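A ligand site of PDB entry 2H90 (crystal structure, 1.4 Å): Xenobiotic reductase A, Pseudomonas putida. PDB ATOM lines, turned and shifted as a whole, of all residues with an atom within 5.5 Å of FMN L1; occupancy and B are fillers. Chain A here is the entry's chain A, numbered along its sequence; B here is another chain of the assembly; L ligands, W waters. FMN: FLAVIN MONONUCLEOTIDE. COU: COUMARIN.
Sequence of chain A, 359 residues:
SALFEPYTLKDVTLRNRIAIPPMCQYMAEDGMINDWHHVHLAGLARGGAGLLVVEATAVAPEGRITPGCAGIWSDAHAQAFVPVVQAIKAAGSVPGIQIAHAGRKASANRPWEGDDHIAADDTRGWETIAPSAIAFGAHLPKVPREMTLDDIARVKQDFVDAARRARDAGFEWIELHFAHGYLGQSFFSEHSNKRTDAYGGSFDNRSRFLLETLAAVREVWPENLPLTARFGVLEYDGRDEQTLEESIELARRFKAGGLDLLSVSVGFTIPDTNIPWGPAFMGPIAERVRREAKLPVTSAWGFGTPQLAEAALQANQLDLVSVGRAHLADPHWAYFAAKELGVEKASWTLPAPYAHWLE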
ATOM      1  N   PRO A  21      12.171  30.263  24.644  1.00  0.00           N
ATOM      2  CA  PRO A  21      13.279  29.933  25.538  1.00  0.00           C
ATOM      3  C   PRO A  21      14.596  30.475  25.020  1.00  0.00           C
ATOM      4  O   PRO A  21      14.722  30.822  23.849  1.00  0.00           O
ATOM      5  CB  PRO A  21      13.252  28.411  25.549  1.00  0.00           C
ATOM      6  CG  PRO A  21      12.884  28.098  24.126  1.00  0.00           C
ATOM      7  CD  PRO A  21      11.775  29.100  23.839  1.00  0.00           C
ATOM      8  N   PRO A  22      15.594  30.559  25.902  1.00  0.00           N
ATOM      9  CA  PRO A  22      16.897  31.071  25.469  1.00  0.00           C
ATOM     10  C   PRO A  22      17.463  30.207  24.353  1.00  0.00           C
ATOM     11  O   PRO A  22      17.414  28.987  24.421  1.00  0.00           O
ATOM     12  CB  PRO A  22      17.729  31.005  26.755  1.00  0.00           C
ATOM     13  CG  PRO A  22      17.067  29.902  27.559  1.00  0.00           C
ATOM     14  CD  PRO A  22      15.614  30.203  27.331  1.00  0.00           C
ATOM     15  N   MET A  23      17.946  30.858  23.299  1.00  0.00           N
ATOM     16  CA  MET A  23      18.535  30.143  22.180  1.00  0.00           C
ATOM     17  C   MET A  23      19.786  30.843  21.672  1.00  0.00           C
ATOM     18  O   MET A  23      19.705  31.879  20.999  1.00  0.00           O
ATOM     19  CB  MET A  23      17.531  29.969  21.038  1.00  0.00           C
ATOM     20  CG  MET A  23      16.420  28.945  21.324  1.00  0.00           C
ATOM     21  SD  MET A  23      15.357  28.667  19.886  1.00  0.00           S
ATOM     22  CE  MET A  23      14.358  30.156  19.935  1.00  0.00           C
ATOM     23  N   CYS A  24      20.942  30.282  22.027  1.00  0.00           N
ATOM     24  CA  CYS A  24      22.232  30.823  21.614  1.00  0.00           C
ATOM     25  C   CYS A  24      22.279  31.029  20.104  1.00  0.00           C
ATOM     26  O   CYS A  24      21.825  30.179  19.327  1.00  0.00           O
ATOM     27  CB  CYS A  24      23.357  29.864  22.010  1.00  0.00           C
ATOM     28  SG  CYS A  24      23.808  29.900  23.752  1.00  0.00           S
ATOM     29  N   GLN A  25      22.856  32.167  19.701  1.00  0.00           N
ATOM     30  CA  GLN A  25      22.988  32.507  18.297  1.00  0.00           C
ATOM     31  C   GLN A  25      24.430  32.386  17.825  1.00  0.00           C
ATOM     32  O   GLN A  25      24.694  32.298  16.628  1.00  0.00           O
ATOM     33  CB  GLN A  25      22.475  33.940  18.071  1.00  0.00           C
ATOM     34  CG  GLN A  25      20.993  34.087  18.393  1.00  0.00           C
ATOM     35  CD  GLN A  25      20.124  33.266  17.461  1.00  0.00           C
ATOM     36  OE1 GLN A  25      19.942  33.601  16.299  1.00  0.00           O
ATOM     37  NE2 GLN A  25      19.587  32.152  17.977  1.00  0.00           N
ATOM     38  N   TYR A  26      25.364  32.365  18.779  1.00  0.00           N
ATOM     39  CA  TYR A  26      26.799  32.234  18.473  1.00  0.00           C
ATOM     40  C   TYR A  26      27.256  33.323  17.498  1.00  0.00           C
ATOM     41  O   TYR A  26      28.144  33.101  16.672  1.00  0.00           O
ATOM     42  CB  TYR A  26      27.057  30.856  17.866  1.00  0.00           C
ATOM     43  CG  TYR A  26      26.529  29.719  18.710  1.00  0.00           C
ATOM     44  CD1 TYR A  26      27.257  29.212  19.781  1.00  0.00           C
ATOM     45  CD2 TYR A  26      25.284  29.162  18.434  1.00  0.00           C
ATOM     46  CE1 TYR A  26      26.755  28.187  20.577  1.00  0.00           C
ATOM     47  CE2 TYR A  26      24.762  28.130  19.218  1.00  0.00           C
ATOM     48  CZ  TYR A  26      25.515  27.641  20.294  1.00  0.00           C
ATOM     49  OH  TYR A  26      25.012  26.626  21.062  1.00  0.00           O
ATOM     50  N   GLU A  55      19.149  34.493  24.900  1.00  0.00           N
ATOM     51  CA  GLU A  55      20.094  33.381  24.984  1.00  0.00           C
ATOM     52  C   GLU A  55      21.053  33.433  26.171  1.00  0.00           C
ATOM     53  O   GLU A  55      21.277  34.498  26.756  1.00  0.00           O
ATOM     54  CB  GLU A  55      20.935  33.348  23.716  1.00  0.00           C
ATOM     55  CG  GLU A  55      21.726  34.635  23.517  1.00  0.00           C
ATOM     56  CD  GLU A  55      22.287  34.754  22.122  1.00  0.00           C
ATOM     57  OE1 GLU A  55      23.321  34.128  21.837  1.00  0.00           O
ATOM     58  OE2 GLU A  55      21.680  35.475  21.309  1.00  0.00           O
ATOM     59  N   ALA A  56      21.620  32.275  26.495  1.00  0.00           N
ATOM     60  CA  ALA A  56      22.580  32.151  27.594  1.00  0.00           C
ATOM     61  C   ALA A  56      23.636  33.237  27.433  1.00  0.00           C
ATOM     62  O   ALA A  56      24.394  33.259  26.456  1.00  0.00           O
ATOM     63  CB  ALA A  56      23.235  30.767  27.549  1.00  0.00           C
ATOM     64  N   GLN A  98      18.696  34.934  30.124  1.00  0.00           N
ATOM     65  CA  GLN A  98      19.262  33.821  30.863  1.00  0.00           C
ATOM     66  C   GLN A  98      20.749  34.135  31.079  1.00  0.00           C
ATOM     67  O   GLN A  98      21.480  34.298  30.117  1.00  0.00           O
ATOM     68  CB  GLN A  98      19.142  32.525  30.054  1.00  0.00           C
ATOM     69  CG  GLN A  98      19.708  31.306  30.769  1.00  0.00           C
ATOM     70  CD  GLN A  98      19.779  30.089  29.880  1.00  0.00           C
ATOM     71  OE1 GLN A  98      20.470  30.097  28.857  1.00  0.00           O
ATOM     72  NE2 GLN A  98      19.074  29.026  30.255  1.00  0.00           N
ATOM     73  N   GLU A 175      16.576  34.510  34.272  1.00  0.00           N
ATOM     74  CA  GLU A 175      16.650  33.067  34.402  1.00  0.00           C
ATOM     75  C   GLU A 175      18.086  32.652  34.667  1.00  0.00           C
ATOM     76  O   GLU A 175      18.970  32.890  33.843  1.00  0.00           O
ATOM     77  CB  GLU A 175      16.139  32.388  33.135  1.00  0.00           C
ATOM     78  CG  GLU A 175      16.168  30.858  33.206  1.00  0.00           C
ATOM     79  CD  GLU A 175      15.771  30.198  31.902  1.00  0.00           C
ATOM     80  OE1 GLU A 175      14.583  30.268  31.524  1.00  0.00           O
ATOM     81  OE2 GLU A 175      16.657  29.621  31.235  1.00  0.00           O
ATOM     82  N   HIS A 177      20.917  30.071  34.712  1.00  0.00           N
ATOM     83  CA  HIS A 177      21.157  28.835  33.983  1.00  0.00           C
ATOM     84  C   HIS A 177      21.830  27.747  34.802  1.00  0.00           C
ATOM     85  O   HIS A 177      23.051  27.600  34.787  1.00  0.00           O
ATOM     86  CB  HIS A 177      21.995  29.127  32.736  1.00  0.00           C
ATOM     87  CG  HIS A 177      21.902  28.065  31.688  1.00  0.00           C
ATOM     88  ND1 HIS A 177      21.305  26.841  31.926  1.00  0.00           N
ATOM     89  CD2 HIS A 177      22.295  28.042  30.395  1.00  0.00           C
ATOM     90  CE1 HIS A 177      21.326  26.123  30.821  1.00  0.00           C
ATOM     91  NE2 HIS A 177      21.916  26.827  29.877  1.00  0.00           N
ATOM     92  N   HIS A 180      21.632  21.873  31.858  1.00  0.00           N
ATOM     93  CA  HIS A 180      22.406  21.414  30.715  1.00  0.00           C
ATOM     94  C   HIS A 180      23.892  21.106  30.887  1.00  0.00           C
ATOM     95  O   HIS A 180      24.676  21.212  29.948  1.00  0.00           O
ATOM     96  CB  HIS A 180      22.161  22.413  29.569  1.00  0.00           C
ATOM     97  CG  HIS A 180      20.703  22.575  29.233  1.00  0.00           C
ATOM     98  ND1 HIS A 180      20.237  23.560  28.389  1.00  0.00           N
ATOM     99  CD2 HIS A 180      19.616  21.867  29.632  1.00  0.00           C
ATOM    100  CE1 HIS A 180      18.923  23.456  28.282  1.00  0.00           C
ATOM    101  NE2 HIS A 180      18.522  22.438  29.027  1.00  0.00           N
ATOM    102  N   ARG A 230      16.642  27.754  35.213  1.00  0.00           N
ATOM    103  CA  ARG A 230      16.453  26.561  34.396  1.00  0.00           C
ATOM    104  C   ARG A 230      17.281  25.518  35.124  1.00  0.00           C
ATOM    105  O   ARG A 230      18.403  25.797  35.553  1.00  0.00           O
ATOM    106  CB  ARG A 230      16.936  26.763  32.955  1.00  0.00           C
ATOM    107  CG  ARG A 230      16.425  25.670  32.026  1.00  0.00           C
ATOM    108  CD  ARG A 230      16.562  26.006  30.546  1.00  0.00           C
ATOM    109  NE  ARG A 230      15.516  25.321  29.786  1.00  0.00           N
ATOM    110  CZ  ARG A 230      15.397  25.357  28.463  1.00  0.00           C
ATOM    111  NH1 ARG A 230      16.269  26.033  27.729  1.00  0.00           N
ATOM    112  NH2 ARG A 230      14.362  24.761  27.878  1.00  0.00           N
ATOM    113  N   ALA A 300      10.225  22.539  27.568  1.00  0.00           N
ATOM    114  CA  ALA A 300      10.265  22.601  26.127  1.00  0.00           C
ATOM    115  C   ALA A 300      10.604  21.260  25.500  1.00  0.00           C
ATOM    116  O   ALA A 300      10.814  20.265  26.195  1.00  0.00           O
ATOM    117  CB  ALA A 300      11.299  23.647  25.701  1.00  0.00           C
ATOM    118  N   TRP A 301      10.643  21.298  24.177  1.00  0.00           N
ATOM    119  CA  TRP A 301      10.959  20.206  23.263  1.00  0.00           C
ATOM    120  C   TRP A 301       9.740  19.624  22.568  1.00  0.00           C
ATOM    121  O   TRP A 301       9.004  18.804  23.128  1.00  0.00           O
ATOM    122  CB  TRP A 301      11.741  19.075  23.931  1.00  0.00           C
ATOM    123  CG  TRP A 301      12.276  18.117  22.901  1.00  0.00           C
ATOM    124  CD1 TRP A 301      11.581  17.129  22.260  1.00  0.00           C
ATOM    125  CD2 TRP A 301      13.585  18.130  22.306  1.00  0.00           C
ATOM    126  NE1 TRP A 301      12.370  16.540  21.295  1.00  0.00           N
ATOM    127  CE2 TRP A 301      13.607  17.138  21.301  1.00  0.00           C
ATOM    128  CE3 TRP A 301      14.745  18.893  22.524  1.00  0.00           C
ATOM    129  CZ2 TRP A 301      14.728  16.888  20.517  1.00  0.00           C
ATOM    130  CZ3 TRP A 301      15.866  18.644  21.740  1.00  0.00           C
ATOM    131  CH2 TRP A 301      15.852  17.649  20.745  1.00  0.00           C
ATOM    132  N   GLY A 302       9.526  20.083  21.331  1.00  0.00           N
ATOM    133  CA  GLY A 302       8.417  19.595  20.530  1.00  0.00           C
ATOM    134  C   GLY A 302       7.083  20.280  20.710  1.00  0.00           C
ATOM    135  O   GLY A 302       6.069  19.775  20.228  1.00  0.00           O
ATOM    136  N   PHE A 303       7.042  21.431  21.378  1.00  0.00           N
ATOM    137  CA  PHE A 303       5.772  22.114  21.578  1.00  0.00           C
ATOM    138  C   PHE A 303       5.424  23.050  20.423  1.00  0.00           C
ATOM    139  O   PHE A 303       4.491  23.841  20.518  1.00  0.00           O
ATOM    140  CB  PHE A 303       5.795  22.881  22.909  1.00  0.00           C
ATOM    141  CG  PHE A 303       5.701  21.992  24.115  1.00  0.00           C
ATOM    142  CD1 PHE A 303       4.484  21.413  24.483  1.00  0.00           C
ATOM    143  CD2 PHE A 303       6.827  21.713  24.888  1.00  0.00           C
ATOM    144  CE1 PHE A 303       4.397  20.584  25.602  1.00  0.00           C
ATOM    145  CE2 PHE A 303       6.748  20.882  25.996  1.00  0.00           C
ATOM    146  CZ  PHE A 303       5.524  20.311  26.357  1.00  0.00           C
ATOM    147  N   GLY A 304       6.171  22.927  19.326  1.00  0.00           N
ATOM    148  CA  GLY A 304       5.921  23.727  18.136  1.00  0.00           C
ATOM    149  C   GLY A 304       4.610  23.329  17.471  1.00  0.00           C
ATOM    150  O   GLY A 304       4.129  24.015  16.561  1.00  0.00           O
ATOM    151  N   SER A 322       7.268  26.689  26.393  1.00  0.00           N
ATOM    152  CA  SER A 322       8.433  27.209  25.691  1.00  0.00           C
ATOM    153  C   SER A 322       8.554  26.566  24.325  1.00  0.00           C
ATOM    154  O   SER A 322       8.594  25.343  24.201  1.00  0.00           O
ATOM    155  CB  SER A 322       9.701  26.964  26.516  1.00  0.00           C
ATOM    156  OG  SER A 322       9.671  27.753  27.697  1.00  0.00           O
ATOM    157  N   VAL A 323       8.611  27.412  23.295  1.00  0.00           N
ATOM    158  CA  VAL A 323       8.709  26.984  21.904  1.00  0.00           C
ATOM    159  C   VAL A 323       9.970  27.581  21.300  1.00  0.00           C
ATOM    160  O   VAL A 323      10.051  28.792  21.071  1.00  0.00           O
ATOM    161  CB  VAL A 323       7.468  27.466  21.114  1.00  0.00           C
ATOM    162  CG1 VAL A 323       7.562  27.035  19.659  1.00  0.00           C
ATOM    163  CG2 VAL A 323       6.199  26.899  21.760  1.00  0.00           C
ATOM    164  N   GLY A 324      10.944  26.728  21.026  1.00  0.00           N
ATOM    165  CA  GLY A 324      12.216  27.201  20.507  1.00  0.00           C
ATOM    166  C   GLY A 324      12.444  27.159  19.009  1.00  0.00           C
ATOM    167  O   GLY A 324      12.254  28.161  18.327  1.00  0.00           O
ATOM    168  N   ARG A 325      12.866  26.000  18.504  1.00  0.00           N
ATOM    169  CA  ARG A 325      13.172  25.862  17.090  1.00  0.00           C
ATOM    170  C   ARG A 325      12.075  26.307  16.129  1.00  0.00           C
ATOM    171  O   ARG A 325      12.368  26.822  15.053  1.00  0.00           O
ATOM    172  CB  ARG A 325      13.599  24.416  16.796  1.00  0.00           C
ATOM    173  CG  ARG A 325      15.044  24.145  17.223  1.00  0.00           C
ATOM    174  CD  ARG A 325      15.391  22.672  17.195  1.00  0.00           C
ATOM    175  NE  ARG A 325      14.618  21.930  18.190  1.00  0.00           N
ATOM    176  CZ  ARG A 325      14.734  20.633  18.410  1.00  0.00           C
ATOM    177  NH1 ARG A 325      15.591  19.911  17.707  1.00  0.00           N
ATOM    178  NH2 ARG A 325      13.973  20.047  19.330  1.00  0.00           N
ATOM    179  N   ALA A 326      10.813  26.137  16.514  1.00  0.00           N
ATOM    180  CA  ALA A 326       9.717  26.551  15.648  1.00  0.00           C
ATOM    181  C   ALA A 326       9.773  28.064  15.402  1.00  0.00           C
ATOM    182  O   ALA A 326       9.283  28.549  14.386  1.00  0.00           O
ATOM    183  CB  ALA A 326       8.375  26.160  16.267  1.00  0.00           C
ATOM    184  N   LEU A 328      12.639  29.712  15.147  1.00  0.00           N
ATOM    185  CA  LEU A 328      13.772  29.980  14.269  1.00  0.00           C
ATOM    186  C   LEU A 328      13.247  29.778  12.851  1.00  0.00           C
ATOM    187  O   LEU A 328      13.610  30.500  11.926  1.00  0.00           O
ATOM    188  CB  LEU A 328      14.931  29.018  14.557  1.00  0.00           C
ATOM    189  CG  LEU A 328      15.471  29.012  15.992  1.00  0.00           C
ATOM    190  CD1 LEU A 328      16.639  28.056  16.082  1.00  0.00           C
ATOM    191  CD2 LEU A 328      15.893  30.422  16.403  1.00  0.00           C
ATOM    192  N   PRO B 353      22.818  30.459  12.104  1.00  0.00           N
ATOM    193  CA  PRO B 353      22.207  30.396  13.434  1.00  0.00           C
ATOM    194  C   PRO B 353      20.823  29.763  13.471  1.00  0.00           C
ATOM    195  O   PRO B 353      20.343  29.374  14.536  1.00  0.00           O
ATOM    196  CB  PRO B 353      22.186  31.860  13.877  1.00  0.00           C
ATOM    197  CG  PRO B 353      23.416  32.406  13.225  1.00  0.00           C
ATOM    198  CD  PRO B 353      23.329  31.809  11.823  1.00  0.00           C
ATOM    199  N   TRP B 357      20.027  24.161  12.974  1.00  0.00           N
ATOM    200  CA  TRP B 357      19.056  23.449  13.802  1.00  0.00           C
ATOM    201  C   TRP B 357      17.785  22.988  13.126  1.00  0.00           C
ATOM    202  O   TRP B 357      17.003  22.252  13.724  1.00  0.00           O
ATOM    203  CB  TRP B 357      18.691  24.338  14.987  1.00  0.00           C
ATOM    204  CG  TRP B 357      19.896  24.998  15.549  1.00  0.00           C
ATOM    205  CD1 TRP B 357      20.337  26.261  15.261  1.00  0.00           C
ATOM    206  CD2 TRP B 357      20.865  24.412  16.402  1.00  0.00           C
ATOM    207  NE1 TRP B 357      21.552  26.488  15.882  1.00  0.00           N
ATOM    208  CE2 TRP B 357      21.893  25.358  16.585  1.00  0.00           C
ATOM    209  CE3 TRP B 357      20.980  23.164  17.027  1.00  0.00           C
ATOM    210  CZ2 TRP B 357      23.020  25.109  17.379  1.00  0.00           C
ATOM    211  CZ3 TRP B 357      22.095  22.903  17.806  1.00  0.00           C
ATOM    212  CH2 TRP B 357      23.104  23.879  17.978  1.00  0.00           C
HETATM  213  N1  FMN L   1      18.738  26.254  26.342  1.00  0.00           N
HETATM  214  C2  FMN L   1      19.217  27.016  27.384  1.00  0.00           C
HETATM  215  O2  FMN L   1      18.943  26.790  28.469  1.00  0.00           O
HETATM  216  N3  FMN L   1      20.105  28.183  26.988  1.00  0.00           N
HETATM  217  C4  FMN L   1      20.491  28.533  25.658  1.00  0.00           C
HETATM  218  O4  FMN L   1      21.201  29.493  25.396  1.00  0.00           O
HETATM  219  C4A FMN L   1      19.967  27.678  24.575  1.00  0.00           C
HETATM  220  N5  FMN L   1      20.276  27.927  23.256  1.00  0.00           N
HETATM  221  C5A FMN L   1      19.781  27.145  22.196  1.00  0.00           C
HETATM  222  C6  FMN L   1      20.194  27.557  20.813  1.00  0.00           C
HETATM  223  C7  FMN L   1      19.676  26.787  19.726  1.00  0.00           C
HETATM  224  C7M FMN L   1      20.125  27.283  18.475  1.00  0.00           C
HETATM  225  C8  FMN L   1      18.691  25.501  19.916  1.00  0.00           C
HETATM  226  C8M FMN L   1      18.124  24.689  18.953  1.00  0.00           C
HETATM  227  C9  FMN L   1      18.375  25.210  21.222  1.00  0.00           C
HETATM  228  C9A FMN L   1      18.860  25.961  22.440  1.00  0.00           C
HETATM  229  N10 FMN L   1      18.547  25.717  23.951  1.00  0.00           N
HETATM  230  C10 FMN L   1      19.054  26.508  25.034  1.00  0.00           C
HETATM  231  C1' FMN L   1      17.646  24.587  24.180  1.00  0.00           C
HETATM  232  C2' FMN L   1      16.200  25.380  23.912  1.00  0.00           C
HETATM  233  O2' FMN L   1      15.928  26.448  24.881  1.00  0.00           O
HETATM  234  C3' FMN L   1      14.978  24.510  24.007  1.00  0.00           C
HETATM  235  O3' FMN L   1      14.788  23.994  25.334  1.00  0.00           O
HETATM  236  C4' FMN L   1      15.120  23.332  22.993  1.00  0.00           C
HETATM  237  O4' FMN L   1      15.337  23.790  21.626  1.00  0.00           O
HETATM  238  C5' FMN L   1      13.892  22.444  22.999  1.00  0.00           C
HETATM  239  O5' FMN L   1      12.659  23.207  22.467  1.00  0.00           O
HETATM  240  P   FMN L   1      12.187  23.143  20.936  1.00  0.00           P
HETATM  241  O1P FMN L   1      13.234  23.684  20.073  1.00  0.00           O
HETATM  242  O2P FMN L   1      11.876  21.698  20.586  1.00  0.00           O
HETATM  243  O3P FMN L   1      10.938  24.044  20.923  1.00  0.00           O
HETATM  244  C1  COU L   2      22.208  25.314  26.104  1.00  0.00           C
HETATM  245  C2  COU L   2      23.145  26.182  25.264  1.00  0.00           C
HETATM  246  C3  COU L   2      23.293  25.972  23.954  1.00  0.00           C
HETATM  247  C4  COU L   2      22.546  24.882  23.270  1.00  0.00           C
HETATM  248  C5  COU L   2      22.653  24.601  21.875  1.00  0.00           C
HETATM  249  C6  COU L   2      21.922  23.552  21.309  1.00  0.00           C
HETATM  250  C7  COU L   2      21.061  22.754  22.119  1.00  0.00           C
HETATM  251  C8  COU L   2      20.931  23.010  23.485  1.00  0.00           C
HETATM  252  C9  COU L   2      21.673  24.069  24.075  1.00  0.00           C
HETATM  253  O1  COU L   2      22.009  25.447  27.295  1.00  0.00           O
HETATM  254  O2  COU L   2      21.501  24.276  25.447  1.00  0.00           O
HETATM  255  O   HOH W   1       9.165  23.126  22.689  1.00  0.00           O
HETATM  256  O   HOH W   2      22.205  29.330  16.705  1.00  0.00           O
HETATM  257  O   HOH W   3      17.468  21.709  21.082  1.00  0.00           O
HETATM  258  O   HOH W   4       9.662  24.435  18.463  1.00  0.00           O
HETATM  259  O   HOH W   5      10.912  20.947  18.173  1.00  0.00           O
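A nitrogen (N3) of FMN L1 lies close to an oxygen (O1) of COU L2, at 3.3 Å.
NE1 of Trp 357 of chain B sits close to O of Pro 353 of chain B (3.4 Å). O of Met 23 lies within hydrogen-bond range of NE2 of Gln 25, 3.0 Å away. NE2 of Gln 98 is in hydrogen-bond range of OE2 of Glu 175, at 2.7 Å. OE1 of Gln 98 lies close to N of Ala 56, 3.4 Å away.
Water W5 bridges O2P of FMN L1 and NH2 of Arg 325. Water W4 lies within hydrogen-bond range of O3P of FMN L1 (2.8 Å) and N of Ala 326 (2.8 Å). Water W2 lies within hydrogen-bond range of O of Cys 24 (2.8 Å), O of Pro 353 of chain B (2.9 Å) and NE1 of Trp 357 of chain B (3.0 Å).
An oxygen (O1P) of FMN L1 lies within hydrogen-bond range of the backbone NH of Arg 325 (2.8 Å). O1 of COU L2 is in hydrogen-bond range of ND1 of His 180, at 2.8 Å. A ring nitrogen (ND1) of His 180 sits close to an oxygen (O2) of FMN L1 (3.5 Å). N5 of FMN L1 lies within hydrogen-bond range of N of Cys 24, at 2.7 Å. The backbone NH of Gly 324 lies within hydrogen-bond range of an oxygen (O3P) of FMN L1 (2.7 Å). NE2 of His 177 sits at hydrogen-bond distance from O1 of COU L2 (2.9 Å). NE of Arg 325 is in salt-bridge range of O1P of FMN L1. The guanidinium group of Arg 230 sits at hydrogen-bond distance from an oxygen (O3') of FMN L1, 2.7 Å away. The backbone carbonyl oxygen (O) of Pro 22 lies close to an oxygen (O2') of FMN L1. The backbone NH (N) of Ala 56 lies within hydrogen-bond range of an oxygen (O4) of FMN L1, 3.0 Å away. The backbone NH (N) of Trp 301 sits at hydrogen-bond distance from an oxygen (O5') of FMN L1, at 3.3 Å. A nitrogen (N3) of FMN L1 is in hydrogen-bond range of the side-chain amide oxygen (OE1) of Gln 98 (2.7 Å). N of Gly 302 is in hydrogen-bond range of O2P of FMN L1, 2.9 Å away. A ring nitrogen (NE2) of His 177 sits at hydrogen-bond distance from an oxygen (O2) of FMN L1 (3.3 Å). SG of Cys 24 is in hydrogen-bond range of O4 of FMN L1 (3.1 Å).
Pro 21 touches FMN L1. Met 23 touches FMN L1. CB of Ala 300 touches O3' of FMN L1 (3.5 Å). Val 323 touches FMN L1 (C to O3P, 3.7 Å). Trp 357 of chain B touches FMN L1 (NE1 to C7M, 3.1 Å). Hydrophobic or aromatic side chains that line FMN L1: Pro 21, Pro 22, Met 23, Ala 56, His 177, His 180, Ala 300, Trp 301 and Trp 357 of chain B. 16 residues have an atom within 4 Å of FMN L1: Pro 21, Pro 22, Met 23, Cys 24, Ala 56, Gln 98, His 177, His 180, Arg 230, Ala 300, Trp 301, Gly 302, Val 323, Gly 324, Arg 325 and Trp 357 of chain B.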
